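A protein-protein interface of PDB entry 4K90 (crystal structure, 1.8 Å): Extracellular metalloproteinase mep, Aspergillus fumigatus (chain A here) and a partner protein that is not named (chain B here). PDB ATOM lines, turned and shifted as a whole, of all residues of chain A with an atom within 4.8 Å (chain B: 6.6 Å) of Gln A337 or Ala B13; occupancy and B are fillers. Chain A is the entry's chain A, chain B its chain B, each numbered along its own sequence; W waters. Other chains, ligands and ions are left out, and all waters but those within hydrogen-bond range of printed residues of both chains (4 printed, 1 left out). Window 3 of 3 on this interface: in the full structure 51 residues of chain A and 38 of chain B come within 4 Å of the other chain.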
ATOM      1  N   PRO A 330     -25.770   2.020   5.258  1.00  0.00           N
ATOM      2  CA  PRO A 330     -25.430   0.668   4.816  1.00  0.00           C
ATOM      3  C   PRO A 330     -26.210  -0.406   5.569  1.00  0.00           C
ATOM      4  O   PRO A 330     -26.869  -0.121   6.558  1.00  0.00           O
ATOM      5  CB  PRO A 330     -23.933   0.536   5.148  1.00  0.00           C
ATOM      6  CG  PRO A 330     -23.663   1.574   6.178  1.00  0.00           C
ATOM      7  CD  PRO A 330     -24.693   2.654   6.054  1.00  0.00           C
ATOM      8  N   CYS A 331     -26.129  -1.637   5.082  1.00  0.00           N
ATOM      9  CA  CYS A 331     -26.700  -2.775   5.757  1.00  0.00           C
ATOM     10  C   CYS A 331     -25.901  -3.000   7.045  1.00  0.00           C
ATOM     11  O   CYS A 331     -24.667  -2.917   7.043  1.00  0.00           O
ATOM     12  CB  CYS A 331     -26.604  -3.986   4.812  1.00  0.00           C
ATOM     13  SG  CYS A 331     -27.336  -5.475   5.414  1.00  0.00           S
ATOM     14  N   ASN A 332     -26.605  -3.289   8.139  1.00  0.00           N
ATOM     15  CA  ASN A 332     -26.015  -3.443   9.489  1.00  0.00           C
ATOM     16  C   ASN A 332     -25.113  -2.281   9.907  1.00  0.00           C
ATOM     17  O   ASN A 332     -23.924  -2.486  10.198  1.00  0.00           O
ATOM     18  CB  ASN A 332     -25.352  -4.808   9.693  1.00  0.00           C
ATOM     19  CG  ASN A 332     -26.383  -5.930   9.777  1.00  0.00           C
ATOM     20  OD1 ASN A 332     -26.385  -6.850   8.956  1.00  0.00           O
ATOM     21  ND2 ASN A 332     -27.280  -5.825  10.723  1.00  0.00           N
ATOM     22  N   PRO A 333     -25.686  -1.066   9.956  1.00  0.00           N
ATOM     23  CA  PRO A 333     -24.917   0.145  10.286  1.00  0.00           C
ATOM     24  C   PRO A 333     -24.643   0.246  11.786  1.00  0.00           C
ATOM     25  O   PRO A 333     -25.343  -0.380  12.588  1.00  0.00           O
ATOM     26  CB  PRO A 333     -25.866   1.277   9.886  1.00  0.00           C
ATOM     27  CG  PRO A 333     -27.233   0.700  10.142  1.00  0.00           C
ATOM     28  CD  PRO A 333     -27.116  -0.754   9.721  1.00  0.00           C
ATOM     29  N   ASN A 334     -23.635   1.037  12.148  1.00  0.00           N
ATOM     30  CA  ASN A 334     -23.398   1.389  13.569  1.00  0.00           C
ATOM     31  C   ASN A 334     -23.973   2.789  13.836  1.00  0.00           C
ATOM     32  O   ASN A 334     -24.450   3.467  12.897  1.00  0.00           O
ATOM     33  CB  ASN A 334     -21.893   1.251  13.917  1.00  0.00           C
ATOM     34  CG  ASN A 334     -21.010   2.247  13.177  1.00  0.00           C
ATOM     35  OD1 ASN A 334     -21.281   3.441  13.169  1.00  0.00           O
ATOM     36  ND2 ASN A 334     -19.917   1.753  12.570  1.00  0.00           N
ATOM     37  N   PHE A 335     -23.976   3.229  15.104  1.00  0.00           N
ATOM     38  CA  PHE A 335     -24.559   4.522  15.461  1.00  0.00           C
ATOM     39  C   PHE A 335     -23.943   5.680  14.674  1.00  0.00           C
ATOM     40  O   PHE A 335     -24.656   6.602  14.295  1.00  0.00           O
ATOM     41  CB  PHE A 335     -24.321   4.846  16.950  1.00  0.00           C
ATOM     42  CG  PHE A 335     -25.306   4.222  17.921  1.00  0.00           C
ATOM     43  CD1 PHE A 335     -25.670   4.934  19.070  1.00  0.00           C
ATOM     44  CD2 PHE A 335     -25.818   2.927  17.750  1.00  0.00           C
ATOM     45  CE1 PHE A 335     -26.545   4.381  20.013  1.00  0.00           C
ATOM     46  CE2 PHE A 335     -26.694   2.356  18.697  1.00  0.00           C
ATOM     47  CZ  PHE A 335     -27.061   3.080  19.829  1.00  0.00           C
ATOM     48  N   VAL A 336     -22.616   5.655  14.496  1.00  0.00           N
ATOM     49  CA  VAL A 336     -21.897   6.763  13.842  1.00  0.00           C
ATOM     50  C   VAL A 336     -22.357   6.889  12.389  1.00  0.00           C
ATOM     51  O   VAL A 336     -22.642   7.991  11.897  1.00  0.00           O
ATOM     52  CB  VAL A 336     -20.378   6.579  13.929  1.00  0.00           C
ATOM     53  CG1 VAL A 336     -19.645   7.705  13.155  1.00  0.00           C
ATOM     54  CG2 VAL A 336     -19.938   6.550  15.413  1.00  0.00           C
ATOM     55  N   GLN A 337     -22.458   5.742  11.723  1.00  0.00           N
ATOM     56  CA  GLN A 337     -22.898   5.688  10.324  1.00  0.00           C
ATOM     57  C   GLN A 337     -24.361   6.132  10.195  1.00  0.00           C
ATOM     58  O   GLN A 337     -24.701   6.901   9.299  1.00  0.00           O
ATOM     59  CB  GLN A 337     -22.717   4.265   9.781  1.00  0.00           C
ATOM     60  CG  GLN A 337     -21.243   3.817   9.734  1.00  0.00           C
ATOM     61  CD  GLN A 337     -21.073   2.333   9.477  1.00  0.00           C
ATOM     62  OE1 GLN A 337     -21.983   1.521   9.716  1.00  0.00           O
ATOM     63  NE2 GLN A 337     -19.891   1.961   9.000  1.00  0.00           N
ATOM     64  N   ALA A 338     -25.221   5.645  11.094  1.00  0.00           N
ATOM     65  CA  ALA A 338     -26.632   6.023  11.070  1.00  0.00           C
ATOM     66  C   ALA A 338     -26.814   7.523  11.328  1.00  0.00           C
ATOM     67  O   ALA A 338     -27.685   8.161  10.714  1.00  0.00           O
ATOM     68  CB  ALA A 338     -27.449   5.185  12.070  1.00  0.00           C
ATOM     69  N   ARG A 339     -25.988   8.073  12.230  1.00  0.00           N
ATOM     70  CA  ARG A 339     -25.959   9.512  12.462  1.00  0.00           C
ATOM     71  C   ARG A 339     -25.597  10.279  11.186  1.00  0.00           C
ATOM     72  O   ARG A 339     -26.319  11.202  10.798  1.00  0.00           O
ATOM     73  CB  ARG A 339     -24.957   9.869  13.574  1.00  0.00           C
ATOM     74  CG  ARG A 339     -24.804  11.382  13.778  1.00  0.00           C
ATOM     75  CD  ARG A 339     -23.471  11.702  14.408  1.00  0.00           C
ATOM     76  NE  ARG A 339     -22.380  11.456  13.477  1.00  0.00           N
ATOM     77  CZ  ARG A 339     -21.106  11.282  13.819  1.00  0.00           C
ATOM     78  NH1 ARG A 339     -20.723  11.318  15.099  1.00  0.00           N
ATOM     79  NH2 ARG A 339     -20.202  11.081  12.868  1.00  0.00           N
ATOM     80  N   ASP A 340     -24.473   9.910  10.565  1.00  0.00           N
ATOM     81  CA  ASP A 340     -24.049  10.516   9.289  1.00  0.00           C
ATOM     82  C   ASP A 340     -25.156  10.432   8.237  1.00  0.00           C
ATOM     83  O   ASP A 340     -25.366  11.381   7.495  1.00  0.00           O
ATOM     84  CB  ASP A 340     -22.762   9.880   8.755  1.00  0.00           C
ATOM     85  CG  ASP A 340     -21.519  10.374   9.488  1.00  0.00           C
ATOM     86  OD1 ASP A 340     -21.668  11.232  10.410  1.00  0.00           O
ATOM     87  OD2 ASP A 340     -20.412   9.901   9.149  1.00  0.00           O
ATOM     88  N   ALA A 341     -25.858   9.295   8.195  1.00  0.00           N
ATOM     89  CA  ALA A 341     -26.959   9.109   7.248  1.00  0.00           C
ATOM     90  C   ALA A 341     -28.109  10.090   7.513  1.00  0.00           C
ATOM     91  O   ALA A 341     -28.738  10.594   6.576  1.00  0.00           O
ATOM     92  CB  ALA A 341     -27.445   7.652   7.269  1.00  0.00           C
ATOM     93  N   LYS B  10     -22.089  -9.509  12.330  1.00  0.00           N
ATOM     94  CA  LYS B  10     -21.272  -8.323  12.652  1.00  0.00           C
ATOM     95  C   LYS B  10     -21.731  -7.003  11.987  1.00  0.00           C
ATOM     96  O   LYS B  10     -22.445  -7.007  10.981  1.00  0.00           O
ATOM     97  CB  LYS B  10     -19.823  -8.620  12.302  1.00  0.00           C
ATOM     98  CG  LYS B  10     -19.278  -9.877  12.964  1.00  0.00           C
ATOM     99  CD  LYS B  10     -19.512  -9.878  14.474  1.00  0.00           C
ATOM    100  CE  LYS B  10     -18.914 -11.127  15.126  1.00  0.00           C
ATOM    101  NZ  LYS B  10     -19.323 -11.278  16.559  1.00  0.00           N
ATOM    102  N   SER B  11     -21.365  -5.869  12.581  1.00  0.00           N
ATOM    103  CA  SER B  11     -21.622  -4.564  11.964  1.00  0.00           C
ATOM    104  C   SER B  11     -20.275  -3.952  11.600  1.00  0.00           C
ATOM    105  O   SER B  11     -19.723  -3.153  12.372  1.00  0.00           O
ATOM    106  CB  SER B  11     -22.454  -3.634  12.874  1.00  0.00           C
ATOM    107  OG  SER B  11     -21.832  -3.381  14.136  1.00  0.00           O
ATOM    108  N   LEU B  12     -19.741  -4.376  10.445  1.00  0.00           N
ATOM    109  CA  LEU B  12     -18.455  -3.887   9.912  1.00  0.00           C
ATOM    110  C   LEU B  12     -18.527  -3.421   8.432  1.00  0.00           C
ATOM    111  O   LEU B  12     -17.526  -3.442   7.690  1.00  0.00           O
ATOM    112  CB  LEU B  12     -17.363  -4.956  10.110  1.00  0.00           C
ATOM    113  CG  LEU B  12     -17.263  -5.591  11.512  1.00  0.00           C
ATOM    114  CD1 LEU B  12     -16.465  -6.897  11.507  1.00  0.00           C
ATOM    115  CD2 LEU B  12     -16.678  -4.623  12.539  1.00  0.00           C
ATOM    116  N   ALA B  13     -19.717  -3.001   8.007  1.00  0.00           N
ATOM    117  CA  ALA B  13     -19.861  -2.198   6.793  1.00  0.00           C
ATOM    118  C   ALA B  13     -19.130  -0.858   6.948  1.00  0.00           C
ATOM    119  O   ALA B  13     -18.815  -0.423   8.071  1.00  0.00           O
ATOM    120  CB  ALA B  13     -21.338  -1.952   6.512  1.00  0.00           C
ATOM    121  N   LYS B  14     -18.850  -0.205   5.823  1.00  0.00           N
ATOM    122  CA  LYS B  14     -18.344   1.149   5.820  1.00  0.00           C
ATOM    123  C   LYS B  14     -19.423   2.040   5.226  1.00  0.00           C
ATOM    124  O   LYS B  14     -20.117   1.622   4.302  1.00  0.00           O
ATOM    125  CB  LYS B  14     -17.074   1.236   4.980  1.00  0.00           C
ATOM    126  CG  LYS B  14     -16.021   0.222   5.415  1.00  0.00           C
ATOM    127  CD  LYS B  14     -14.821   0.182   4.491  1.00  0.00           C
ATOM    128  N   TYR B  15     -19.571   3.251   5.758  1.00  0.00           N
ATOM    129  CA  TYR B  15     -20.433   4.248   5.130  1.00  0.00           C
ATOM    130  C   TYR B  15     -19.566   5.421   4.756  1.00  0.00           C
ATOM    131  O   TYR B  15     -18.992   6.065   5.643  1.00  0.00           O
ATOM    132  CB  TYR B  15     -21.545   4.738   6.071  1.00  0.00           C
ATOM    133  CG  TYR B  15     -22.465   5.791   5.447  1.00  0.00           C
ATOM    134  CD1 TYR B  15     -23.190   5.514   4.276  1.00  0.00           C
ATOM    135  CD2 TYR B  15     -22.612   7.059   6.031  1.00  0.00           C
ATOM    136  CE1 TYR B  15     -24.024   6.480   3.687  1.00  0.00           C
ATOM    137  CE2 TYR B  15     -23.464   8.049   5.452  1.00  0.00           C
ATOM    138  CZ  TYR B  15     -24.158   7.742   4.274  1.00  0.00           C
ATOM    139  OH  TYR B  15     -24.969   8.693   3.696  1.00  0.00           O
ATOM    140  N   ASP B  85     -22.481  -6.534   0.533  1.00  0.00           N
ATOM    141  CA  ASP B  85     -23.433  -5.611  -0.075  1.00  0.00           C
ATOM    142  C   ASP B  85     -22.758  -4.295  -0.394  1.00  0.00           C
ATOM    143  O   ASP B  85     -21.782  -3.926   0.256  1.00  0.00           O
ATOM    144  CB  ASP B  85     -24.573  -5.357   0.908  1.00  0.00           C
ATOM    145  CG  ASP B  85     -25.244  -6.646   1.357  1.00  0.00           C
ATOM    146  OD1 ASP B  85     -25.859  -7.297   0.499  1.00  0.00           O
ATOM    147  OD2 ASP B  85     -25.130  -7.014   2.554  1.00  0.00           O
ATOM    148  N   GLY B 100     -22.404   2.966   0.849  1.00  0.00           N
ATOM    149  CA  GLY B 100     -21.934   2.068   1.887  1.00  0.00           C
ATOM    150  C   GLY B 100     -21.436   0.815   1.217  1.00  0.00           C
ATOM    151  O   GLY B 100     -21.826   0.494   0.075  1.00  0.00           O
ATOM    152  N   ASN B 101     -20.563   0.086   1.887  1.00  0.00           N
ATOM    153  CA  ASN B 101     -20.274  -1.224   1.371  1.00  0.00           C
ATOM    154  C   ASN B 101     -19.564  -2.164   2.309  1.00  0.00           C
ATOM    155  O   ASN B 101     -18.857  -1.739   3.237  1.00  0.00           O
ATOM    156  CB  ASN B 101     -19.614  -1.144   0.001  1.00  0.00           C
ATOM    157  CG  ASN B 101     -18.134  -1.200   0.064  1.00  0.00           C
ATOM    158  OD1 ASN B 101     -17.539  -2.184  -0.365  1.00  0.00           O
ATOM    159  ND2 ASN B 101     -17.520  -0.154   0.596  1.00  0.00           N
ATOM    160  N   SER B 102     -19.807  -3.444   2.063  1.00  0.00           N
ATOM    161  CA  SER B 102     -19.207  -4.508   2.826  1.00  0.00           C
ATOM    162  C   SER B 102     -18.658  -5.559   1.867  1.00  0.00           C
ATOM    163  O   SER B 102     -18.639  -6.737   2.196  1.00  0.00           O
ATOM    164  CB  SER B 102     -20.240  -5.115   3.769  1.00  0.00           C
ATOM    165  OG  SER B 102     -21.374  -5.596   3.058  1.00  0.00           O
HETATM  166  O   HOH W   1     -21.464  -1.190  10.044  1.00  0.00           O
HETATM  167  O   HOH W   2     -19.169  -0.804  11.447  1.00  0.00           O
HETATM  168  O   HOH W   3     -20.120   7.494   8.302  1.00  0.00           O
HETATM  169  O   HOH W   4     -17.742   3.814   8.026  1.00  0.00           O
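O of Ala B13 is in hydrogen-bond range of NE2 of Gln A337 (2.8 Å).
The side-chain amide oxygen of Asn A334 sits at hydrogen-bond distance from the backbone NH of Gln A337, at 3.0 Å. The side-chain carboxylate (OD1) of Asp A340 lies within salt-bridge range of the guanidinium group (NH2) of Arg A339, at 2.9 Å. O of Lys B14 is in hydrogen-bond range of N of Asn B101 (2.9 Å). The backbone carbonyl oxygen (O) of Asp B85 sits at hydrogen-bond distance from the backbone NH (N) of Ser B102 (2.7 Å).
Among the printed residues, pairs that only touch across the chains: Pro A330 with Ala B13 (3.8 Å), Pro A330 with Tyr B15 (3.7 Å), Cys A331 with Ala B13 (3.5 Å), Cys A331 with Asp B85 (3.9 Å), Asn A332 with Lys B10 (3.9 Å), Asn A332 with Ser B11 (3.3 Å), Gln A337 with Lys B14 (3.6 Å), Gln A337 with Tyr B15 (3.5 Å), Asp A340 with Tyr B15 (3.8 Å) and Ala A341 with Tyr B15 (3.8 Å).
Of the printed residues of chain B, Pro A330 touches Ala B13 (3.8 Å) and Tyr B15 (3.7 Å). Asn A334 touches none of the printed residues of chain B. Gln A337 touches three residues of chain B. Printed residues of chain B within 4 Å of Ala A341: Tyr B15. Printed residues of chain A within 4 Å of Lys B14: Gln A337 (3.6 Å). Printed residues of chain A within 4 Å of Tyr B15: Pro A330 (3.7 Å), Gln A337 (3.5 Å), Asp A340 (3.8 Å) and Ala A341 (3.8 Å). Of the printed residues of chain A, Asp B85 touches Cys A331. Ser B102 touches none of the printed residues of chain A. The nearest printed residue of chain B that does not touch Asn A332 is Ala B13 (4.5 Å).
Of the 12 printed residues of chain A, 6 touch a printed residue of chain B. Hydrophobic or aromatic side chains of chain B within 4 Å of the printed part of chain A: Ala B13 and Tyr B15. Among the printed residues, 11 pairs touch across the chains.
Water W3 bridges OD2 of Asp A340 and O of Tyr B15. Water W2 lies within hydrogen-bond range of O of Ser B11 (2.6 Å), ND2 of Asn A334 (2.9 Å) and O of Ala B13 (3.4 Å). Water W1 lies within hydrogen-bond range of OE1 of Gln A337, O of Asn A332 and N of Ala B13. Water W4 bridges the backbone NH (N) of Tyr B15 and the side-chain amide nitrogen (NE2) of Gln A337.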
